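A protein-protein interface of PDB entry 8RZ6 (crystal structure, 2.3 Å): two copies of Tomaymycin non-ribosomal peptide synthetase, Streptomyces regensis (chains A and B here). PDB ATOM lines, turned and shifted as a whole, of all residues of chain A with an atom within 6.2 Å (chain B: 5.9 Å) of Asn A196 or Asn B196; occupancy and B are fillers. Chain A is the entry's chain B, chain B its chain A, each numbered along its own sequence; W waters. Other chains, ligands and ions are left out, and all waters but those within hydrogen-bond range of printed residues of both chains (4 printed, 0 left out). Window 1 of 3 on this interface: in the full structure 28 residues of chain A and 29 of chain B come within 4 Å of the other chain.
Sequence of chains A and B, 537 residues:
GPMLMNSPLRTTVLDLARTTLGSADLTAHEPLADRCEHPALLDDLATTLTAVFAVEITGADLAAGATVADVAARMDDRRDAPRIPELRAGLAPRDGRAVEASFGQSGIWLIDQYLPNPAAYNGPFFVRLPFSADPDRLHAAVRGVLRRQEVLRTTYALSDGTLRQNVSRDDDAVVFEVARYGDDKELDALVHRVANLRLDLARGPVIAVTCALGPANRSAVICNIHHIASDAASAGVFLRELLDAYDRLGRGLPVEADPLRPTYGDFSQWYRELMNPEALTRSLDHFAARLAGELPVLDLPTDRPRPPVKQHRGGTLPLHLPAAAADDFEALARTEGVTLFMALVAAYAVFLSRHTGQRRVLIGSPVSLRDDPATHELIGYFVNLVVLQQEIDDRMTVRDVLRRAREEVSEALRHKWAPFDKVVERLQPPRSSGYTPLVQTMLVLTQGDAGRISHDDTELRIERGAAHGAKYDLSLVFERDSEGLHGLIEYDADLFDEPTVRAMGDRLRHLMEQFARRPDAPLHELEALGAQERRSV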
ATOM      1  N   PRO A 116      18.824   4.279 -25.074  1.00  0.00           N
ATOM      2  CA  PRO A 116      19.395   2.939 -25.259  1.00  0.00           C
ATOM      3  C   PRO A 116      18.382   1.973 -25.875  1.00  0.00           C
ATOM      4  O   PRO A 116      17.170   2.226 -25.974  1.00  0.00           O
ATOM      5  CB  PRO A 116      19.769   2.503 -23.830  1.00  0.00           C
ATOM      6  CG  PRO A 116      19.752   3.742 -23.003  1.00  0.00           C
ATOM      7  CD  PRO A 116      18.747   4.664 -23.654  1.00  0.00           C
ATOM      8  N   ASN A 117      18.888   0.816 -26.253  1.00  0.00           N
ATOM      9  CA  ASN A 117      17.985  -0.257 -26.632  1.00  0.00           C
ATOM     10  C   ASN A 117      17.009  -0.512 -25.478  1.00  0.00           C
ATOM     11  O   ASN A 117      17.437  -0.558 -24.309  1.00  0.00           O
ATOM     12  CB  ASN A 117      18.777  -1.516 -26.976  1.00  0.00           C
ATOM     13  CG  ASN A 117      19.791  -1.860 -25.913  1.00  0.00           C
ATOM     14  OD1 ASN A 117      20.731  -1.085 -25.653  1.00  0.00           O
ATOM     15  ND2 ASN A 117      19.581  -2.998 -25.245  1.00  0.00           N
ATOM     16  N   PRO A 124      21.651  -5.731 -28.489  1.00  0.00           N
ATOM     17  CA  PRO A 124      22.989  -6.064 -29.015  1.00  0.00           C
ATOM     18  C   PRO A 124      23.476  -7.435 -28.583  1.00  0.00           C
ATOM     19  O   PRO A 124      23.250  -7.872 -27.444  1.00  0.00           O
ATOM     20  CB  PRO A 124      23.884  -4.959 -28.442  1.00  0.00           C
ATOM     21  CG  PRO A 124      22.942  -3.767 -28.284  1.00  0.00           C
ATOM     22  CD  PRO A 124      21.567  -4.356 -27.967  1.00  0.00           C
ATOM     23  N   VAL A 191      31.829  -5.200 -26.364  1.00  0.00           N
ATOM     24  CA  VAL A 191      30.361  -5.334 -26.438  1.00  0.00           C
ATOM     25  C   VAL A 191      29.668  -4.062 -25.937  1.00  0.00           C
ATOM     26  O   VAL A 191      28.698  -3.575 -26.548  1.00  0.00           O
ATOM     27  CB  VAL A 191      29.907  -6.581 -25.641  1.00  0.00           C
ATOM     28  CG1 VAL A 191      28.403  -6.605 -25.438  1.00  0.00           C
ATOM     29  CG2 VAL A 191      30.396  -7.877 -26.316  1.00  0.00           C
ATOM     30  N   HIS A 192      30.143  -3.510 -24.800  1.00  0.00           N
ATOM     31  CA  HIS A 192      29.510  -2.312 -24.239  1.00  0.00           C
ATOM     32  C   HIS A 192      29.606  -1.137 -25.204  1.00  0.00           C
ATOM     33  O   HIS A 192      28.664  -0.346 -25.332  1.00  0.00           O
ATOM     34  CB  HIS A 192      30.131  -1.925 -22.878  1.00  0.00           C
ATOM     35  CG  HIS A 192      29.606  -2.735 -21.729  1.00  0.00           C
ATOM     36  ND1 HIS A 192      30.402  -3.592 -20.995  1.00  0.00           N
ATOM     37  CD2 HIS A 192      28.363  -2.836 -21.202  1.00  0.00           C
ATOM     38  CE1 HIS A 192      29.669  -4.202 -20.081  1.00  0.00           C
ATOM     39  NE2 HIS A 192      28.433  -3.739 -20.167  1.00  0.00           N
ATOM     40  N   ARG A 193      30.736  -0.994 -25.889  1.00  0.00           N
ATOM     41  CA  ARG A 193      30.852   0.134 -26.807  1.00  0.00           C
ATOM     42  C   ARG A 193      29.854  -0.007 -27.951  1.00  0.00           C
ATOM     43  O   ARG A 193      29.194   0.965 -28.337  1.00  0.00           O
ATOM     44  CB  ARG A 193      32.292   0.249 -27.323  1.00  0.00           C
ATOM     45  CG  ARG A 193      32.444   1.140 -28.503  1.00  0.00           C
ATOM     46  CD  ARG A 193      33.892   1.685 -28.624  1.00  0.00           C
ATOM     47  NE  ARG A 193      34.875   0.705 -29.069  1.00  0.00           N
ATOM     48  CZ  ARG A 193      35.997   0.396 -28.432  1.00  0.00           C
ATOM     49  NH1 ARG A 193      36.242   0.825 -27.220  1.00  0.00           N
ATOM     50  NH2 ARG A 193      36.913  -0.347 -29.042  1.00  0.00           N
ATOM     51  N   VAL A 194      29.735  -1.208 -28.510  1.00  0.00           N
ATOM     52  CA  VAL A 194      28.747  -1.447 -29.562  1.00  0.00           C
ATOM     53  C   VAL A 194      27.349  -1.231 -29.023  1.00  0.00           C
ATOM     54  O   VAL A 194      26.497  -0.631 -29.685  1.00  0.00           O
ATOM     55  CB  VAL A 194      28.908  -2.867 -30.122  1.00  0.00           C
ATOM     56  CG1 VAL A 194      27.690  -3.247 -30.994  1.00  0.00           C
ATOM     57  CG2 VAL A 194      30.206  -2.965 -30.899  1.00  0.00           C
ATOM     58  N   ALA A 195      27.090  -1.733 -27.811  1.00  0.00           N
ATOM     59  CA  ALA A 195      25.736  -1.733 -27.269  1.00  0.00           C
ATOM     60  C   ALA A 195      25.239  -0.335 -26.930  1.00  0.00           C
ATOM     61  O   ALA A 195      24.026  -0.110 -26.868  1.00  0.00           O
ATOM     62  CB  ALA A 195      25.665  -2.614 -26.009  1.00  0.00           C
ATOM     63  N   ASN A 196      26.134   0.612 -26.688  1.00  0.00           N
ATOM     64  CA  ASN A 196      25.725   1.938 -26.266  1.00  0.00           C
ATOM     65  C   ASN A 196      25.671   2.934 -27.433  1.00  0.00           C
ATOM     66  O   ASN A 196      25.430   4.121 -27.203  1.00  0.00           O
ATOM     67  CB  ASN A 196      26.659   2.427 -25.143  1.00  0.00           C
ATOM     68  CG  ASN A 196      26.642   1.506 -23.891  1.00  0.00           C
ATOM     69  OD1 ASN A 196      27.680   1.282 -23.271  1.00  0.00           O
ATOM     70  ND2 ASN A 196      25.467   0.979 -23.529  1.00  0.00           N
ATOM     71  N   LEU A 197      25.829   2.474 -28.677  1.00  0.00           N
ATOM     72  CA  LEU A 197      25.663   3.370 -29.822  1.00  0.00           C
ATOM     73  C   LEU A 197      24.209   3.846 -29.876  1.00  0.00           C
ATOM     74  O   LEU A 197      23.296   3.147 -29.440  1.00  0.00           O
ATOM     75  CB  LEU A 197      26.023   2.658 -31.121  1.00  0.00           C
ATOM     76  CG  LEU A 197      27.456   2.185 -31.219  1.00  0.00           C
ATOM     77  CD1 LEU A 197      27.629   1.328 -32.438  1.00  0.00           C
ATOM     78  CD2 LEU A 197      28.346   3.377 -31.338  1.00  0.00           C
ATOM     79  N   ARG A 198      23.990   5.050 -30.383  1.00  0.00           N
ATOM     80  CA  ARG A 198      22.652   5.639 -30.477  1.00  0.00           C
ATOM     81  C   ARG A 198      22.502   5.965 -31.962  1.00  0.00           C
ATOM     82  O   ARG A 198      22.902   7.035 -32.431  1.00  0.00           O
ATOM     83  CB  ARG A 198      22.474   6.868 -29.576  1.00  0.00           C
ATOM     84  CG  ARG A 198      22.860   6.644 -28.095  1.00  0.00           C
ATOM     85  CD  ARG A 198      21.879   5.747 -27.312  1.00  0.00           C
ATOM     86  NE  ARG A 198      22.389   5.393 -25.984  1.00  0.00           N
ATOM     87  CZ  ARG A 198      22.109   6.045 -24.857  1.00  0.00           C
ATOM     88  NH1 ARG A 198      21.300   7.104 -24.834  1.00  0.00           N
ATOM     89  NH2 ARG A 198      22.647   5.620 -23.719  1.00  0.00           N
ATOM     90  N   ASN A 224      25.068  -4.646 -33.318  1.00  0.00           N
ATOM     91  CA  ASN A 224      23.932  -3.866 -32.863  1.00  0.00           C
ATOM     92  C   ASN A 224      23.082  -3.512 -34.069  1.00  0.00           C
ATOM     93  O   ASN A 224      23.542  -2.780 -34.950  1.00  0.00           O
ATOM     94  CB  ASN A 224      24.404  -2.601 -32.146  1.00  0.00           C
ATOM     95  CG  ASN A 224      23.262  -1.786 -31.544  1.00  0.00           C
ATOM     96  OD1 ASN A 224      22.078  -2.022 -31.806  1.00  0.00           O
ATOM     97  ND2 ASN A 224      23.641  -0.784 -30.722  1.00  0.00           N
ATOM     98  N   GLN A 311      16.236   7.726 -16.227  1.00  0.00           N
ATOM     99  CA  GLN A 311      17.658   7.661 -16.590  1.00  0.00           C
ATOM    100  C   GLN A 311      17.986   6.505 -17.521  1.00  0.00           C
ATOM    101  O   GLN A 311      19.149   6.357 -17.940  1.00  0.00           O
ATOM    102  CB  GLN A 311      18.514   7.559 -15.322  1.00  0.00           C
ATOM    103  CG  GLN A 311      18.373   8.770 -14.387  1.00  0.00           C
ATOM    104  CD  GLN A 311      18.927  10.082 -14.998  1.00  0.00           C
ATOM    105  OE1 GLN A 311      19.635  10.086 -16.028  1.00  0.00           O
ATOM    106  NE2 GLN A 311      18.614  11.184 -14.356  1.00  0.00           N
ATOM    107  N   ALA A 467      23.107  -4.638 -21.082  1.00  0.00           N
ATOM    108  CA  ALA A 467      22.724  -3.255 -20.889  1.00  0.00           C
ATOM    109  C   ALA A 467      21.479  -2.959 -21.695  1.00  0.00           C
ATOM    110  O   ALA A 467      21.358  -3.409 -22.841  1.00  0.00           O
ATOM    111  CB  ALA A 467      23.849  -2.311 -21.320  1.00  0.00           C
ATOM    112  N   PRO B 116      27.601  11.188 -24.647  1.00  0.00           N
ATOM    113  CA  PRO B 116      28.414  10.619 -23.568  1.00  0.00           C
ATOM    114  C   PRO B 116      29.456  11.628 -23.090  1.00  0.00           C
ATOM    115  O   PRO B 116      29.676  12.699 -23.684  1.00  0.00           O
ATOM    116  CB  PRO B 116      29.040   9.367 -24.201  1.00  0.00           C
ATOM    117  CG  PRO B 116      28.896   9.548 -25.673  1.00  0.00           C
ATOM    118  CD  PRO B 116      27.731  10.450 -25.919  1.00  0.00           C
ATOM    119  N   ASN B 117      30.077  11.293 -21.963  1.00  0.00           N
ATOM    120  CA  ASN B 117      31.187  12.091 -21.479  1.00  0.00           C
ATOM    121  C   ASN B 117      32.234  12.273 -22.589  1.00  0.00           C
ATOM    122  O   ASN B 117      32.655  11.280 -23.217  1.00  0.00           O
ATOM    123  CB  ASN B 117      31.796  11.428 -20.245  1.00  0.00           C
ATOM    124  CG  ASN B 117      32.120   9.959 -20.463  1.00  0.00           C
ATOM    125  OD1 ASN B 117      31.217   9.115 -20.694  1.00  0.00           O
ATOM    126  ND2 ASN B 117      33.432   9.639 -20.417  1.00  0.00           N
ATOM    127  N   PRO B 124      33.662   9.481 -15.715  1.00  0.00           N
ATOM    128  CA  PRO B 124      33.209   8.576 -14.644  1.00  0.00           C
ATOM    129  C   PRO B 124      34.364   7.820 -14.010  1.00  0.00           C
ATOM    130  O   PRO B 124      35.278   7.377 -14.699  1.00  0.00           O
ATOM    131  CB  PRO B 124      32.245   7.623 -15.364  1.00  0.00           C
ATOM    132  CG  PRO B 124      31.672   8.455 -16.495  1.00  0.00           C
ATOM    133  CD  PRO B 124      32.792   9.425 -16.916  1.00  0.00           C
ATOM    134  N   VAL B 191      30.306  -0.169 -13.600  1.00  0.00           N
ATOM    135  CA  VAL B 191      30.910   1.095 -14.031  1.00  0.00           C
ATOM    136  C   VAL B 191      30.327   1.558 -15.372  1.00  0.00           C
ATOM    137  O   VAL B 191      30.028   2.751 -15.569  1.00  0.00           O
ATOM    138  CB  VAL B 191      32.444   0.926 -14.106  1.00  0.00           C
ATOM    139  CG1 VAL B 191      33.066   2.140 -14.818  1.00  0.00           C
ATOM    140  CG2 VAL B 191      33.060   0.695 -12.708  1.00  0.00           C
ATOM    141  N   HIS B 192      30.157   0.621 -16.317  1.00  0.00           N
ATOM    142  CA  HIS B 192      29.587   0.981 -17.616  1.00  0.00           C
ATOM    143  C   HIS B 192      28.177   1.531 -17.469  1.00  0.00           C
ATOM    144  O   HIS B 192      27.809   2.528 -18.098  1.00  0.00           O
ATOM    145  CB  HIS B 192      29.598  -0.225 -18.568  1.00  0.00           C
ATOM    146  CG  HIS B 192      30.926  -0.462 -19.211  1.00  0.00           C
ATOM    147  ND1 HIS B 192      31.658  -1.614 -19.010  1.00  0.00           N
ATOM    148  CD2 HIS B 192      31.654   0.301 -20.061  1.00  0.00           C
ATOM    149  CE1 HIS B 192      32.787  -1.541 -19.691  1.00  0.00           C
ATOM    150  NE2 HIS B 192      32.803  -0.395 -20.347  1.00  0.00           N
ATOM    151  N   ARG B 193      27.373   0.924 -16.613  1.00  0.00           N
ATOM    152  CA  ARG B 193      26.031   1.462 -16.448  1.00  0.00           C
ATOM    153  C   ARG B 193      26.096   2.901 -15.941  1.00  0.00           C
ATOM    154  O   ARG B 193      25.454   3.799 -16.492  1.00  0.00           O
ATOM    155  CB  ARG B 193      25.213   0.562 -15.510  1.00  0.00           C
ATOM    156  CG  ARG B 193      23.874   1.152 -15.076  1.00  0.00           C
ATOM    157  CD  ARG B 193      22.882   0.046 -14.733  1.00  0.00           C
ATOM    158  NE  ARG B 193      23.119  -0.572 -13.438  1.00  0.00           N
ATOM    159  CZ  ARG B 193      23.221  -1.876 -13.212  1.00  0.00           C
ATOM    160  NH1 ARG B 193      23.274  -2.746 -14.196  1.00  0.00           N
ATOM    161  NH2 ARG B 193      23.258  -2.321 -11.952  1.00  0.00           N
ATOM    162  N   VAL B 194      26.899   3.145 -14.906  1.00  0.00           N
ATOM    163  CA  VAL B 194      27.021   4.501 -14.371  1.00  0.00           C
ATOM    164  C   VAL B 194      27.597   5.431 -15.422  1.00  0.00           C
ATOM    165  O   VAL B 194      27.139   6.564 -15.574  1.00  0.00           O
ATOM    166  CB  VAL B 194      27.883   4.512 -13.098  1.00  0.00           C
ATOM    167  CG1 VAL B 194      28.238   5.953 -12.721  1.00  0.00           C
ATOM    168  CG2 VAL B 194      27.154   3.824 -11.951  1.00  0.00           C
ATOM    169  N   ALA B 195      28.601   4.959 -16.178  1.00  0.00           N
ATOM    170  CA  ALA B 195      29.332   5.857 -17.059  1.00  0.00           C
ATOM    171  C   ALA B 195      28.506   6.263 -18.265  1.00  0.00           C
ATOM    172  O   ALA B 195      28.761   7.309 -18.858  1.00  0.00           O
ATOM    173  CB  ALA B 195      30.637   5.205 -17.517  1.00  0.00           C
ATOM    174  N   ASN B 196      27.521   5.466 -18.651  1.00  0.00           N
ATOM    175  CA  ASN B 196      26.737   5.751 -19.839  1.00  0.00           C
ATOM    176  C   ASN B 196      25.421   6.491 -19.534  1.00  0.00           C
ATOM    177  O   ASN B 196      24.638   6.738 -20.455  1.00  0.00           O
ATOM    178  CB  ASN B 196      26.478   4.443 -20.606  1.00  0.00           C
ATOM    179  CG  ASN B 196      27.780   3.720 -21.038  1.00  0.00           C
ATOM    180  OD1 ASN B 196      27.873   2.491 -20.916  1.00  0.00           O
ATOM    181  ND2 ASN B 196      28.772   4.472 -21.556  1.00  0.00           N
ATOM    182  N   LEU B 197      25.194   6.920 -18.290  1.00  0.00           N
ATOM    183  CA  LEU B 197      24.071   7.808 -18.026  1.00  0.00           C
ATOM    184  C   LEU B 197      24.266   9.101 -18.818  1.00  0.00           C
ATOM    185  O   LEU B 197      25.399   9.523 -19.075  1.00  0.00           O
ATOM    186  CB  LEU B 197      23.966   8.117 -16.542  1.00  0.00           C
ATOM    187  CG  LEU B 197      23.788   6.890 -15.652  1.00  0.00           C
ATOM    188  CD1 LEU B 197      23.909   7.237 -14.209  1.00  0.00           C
ATOM    189  CD2 LEU B 197      22.425   6.333 -15.948  1.00  0.00           C
ATOM    190  N   ARG B 198      23.159   9.727 -19.210  1.00  0.00           N
ATOM    191  CA  ARG B 198      23.151  10.986 -19.958  1.00  0.00           C
ATOM    192  C   ARG B 198      22.317  11.944 -19.111  1.00  0.00           C
ATOM    193  O   ARG B 198      21.092  12.001 -19.240  1.00  0.00           O
ATOM    194  CB  ARG B 198      22.566  10.842 -21.370  1.00  0.00           C
ATOM    195  CG  ARG B 198      23.122   9.681 -22.193  1.00  0.00           C
ATOM    196  CD  ARG B 198      24.548   9.941 -22.670  1.00  0.00           C
ATOM    197  NE  ARG B 198      25.112   8.742 -23.292  1.00  0.00           N
ATOM    198  CZ  ARG B 198      25.070   8.452 -24.594  1.00  0.00           C
ATOM    199  NH1 ARG B 198      24.544   9.286 -25.490  1.00  0.00           N
ATOM    200  NH2 ARG B 198      25.570   7.294 -25.014  1.00  0.00           N
ATOM    201  N   ASN B 224      29.582   9.296 -11.381  1.00  0.00           N
ATOM    202  CA  ASN B 224      29.540  10.086 -12.593  1.00  0.00           C
ATOM    203  C   ASN B 224      29.071  11.480 -12.215  1.00  0.00           C
ATOM    204  O   ASN B 224      27.958  11.646 -11.685  1.00  0.00           O
ATOM    205  CB  ASN B 224      28.584   9.426 -13.596  1.00  0.00           C
ATOM    206  CG  ASN B 224      28.611  10.081 -14.966  1.00  0.00           C
ATOM    207  OD1 ASN B 224      29.246  11.113 -15.169  1.00  0.00           O
ATOM    208  ND2 ASN B 224      27.891   9.466 -15.929  1.00  0.00           N
ATOM    209  N   ALA B 467      35.189   4.335 -21.286  1.00  0.00           N
ATOM    210  CA  ALA B 467      34.241   4.730 -22.313  1.00  0.00           C
ATOM    211  C   ALA B 467      34.100   6.244 -22.372  1.00  0.00           C
ATOM    212  O   ALA B 467      34.040   6.917 -21.339  1.00  0.00           O
ATOM    213  CB  ALA B 467      32.869   4.105 -22.049  1.00  0.00           C
HETATM  214  O   HOH W   1      20.712   8.779 -18.310  1.00  0.00           O
HETATM  215  O   HOH W   2      25.730   0.424 -20.174  1.00  0.00           O
HETATM  216  O   HOH W   3      21.698   5.311 -19.435  1.00  0.00           O
HETATM  217  O   HOH W   4      18.718  12.390 -17.877  1.00  0.00           O
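ND1 of His B192 is in hydrogen-bond range of ND1 of His A192, at 3.1 Å. The side-chain amide oxygen (OD1) of Asn B196 sits close to the side-chain amide oxygen (OD1) of Asn A196 (2.7 Å).
The side-chain amide oxygen (OD1) of Asn B196 sits close to the backbone carbonyl oxygen (O) of His B192 (2.8 Å). The side-chain amide oxygen (OD1) of Asn A196 sits close to the backbone carbonyl oxygen (O) of His A192, 2.8 Å away.
Arg B198 touches Asn A196. Asn B196 touches Arg A198 (O to NH2, 3.98 Å). Arg A198 touches Arg B198 (NH2 to NH2, 3.6 Å). Leu B197 touches Gln A311 (CD2 to O, 3.8 Å).
Of the printed residues of chain B, Asn A196 touches Asn B196 and Arg B198. Of the printed residues of chain A, Asn B196 touches Asn A196 and Arg A198. Of the printed residues of chain A, Arg B198 touches Asn A196 (3.9 Å) and Arg A198 (3.6 Å). Printed residues of chain A within 4 Å of Leu B197: Gln A311 (3.8 Å). Val B191 touches none of the printed residues of chain A. The nearest printed residue of chain B that does not touch Asn A196 is His B192 (5.2 Å). The nearest printed residue of chain B that does not touch His A192 is Asn B196 (5.3 Å).
Hydrophobic or aromatic side chains of chain B that line the printed part of chain A: His B192 and Leu B197. Of the 14 printed residues of chain A, 4 touch a printed residue of chain B. Among the printed residues, 6 pairs touch across the chains. Among the printed residues, no Asp or Glu carboxylate lies within 4 Å of a Lys or Arg side-chain nitrogen of the other chain.
His B192 touches its own counterpart, His A192. Asn B196 touches its own counterpart, Asn A196. Asn A196 touches Arg B198, and with the chains exchanged Arg A198 touches Asn B196. Arg A198 touches its own counterpart, Arg B198. Of the 6 pairs that touch across the chains among the printed residues, 5 have their exchanged pair printed and touching as well.
Water W4 bridges the backbone carbonyl oxygen (O) of Arg B198 (2.8 Å) and the side-chain amide oxygen (OE1) of Gln A311 (3.1 Å). Water W1 bridges the backbone NH (N) of Arg B198 and the side-chain amide oxygen (OE1) of Gln A311. Water W2 bridges OD1 of Asn B196 and ND2 of Asn A196. Water W3 lies within hydrogen-bond range of the backbone carbonyl oxygen of Gln A311 and the backbone carbonyl oxygen of Asn B196.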
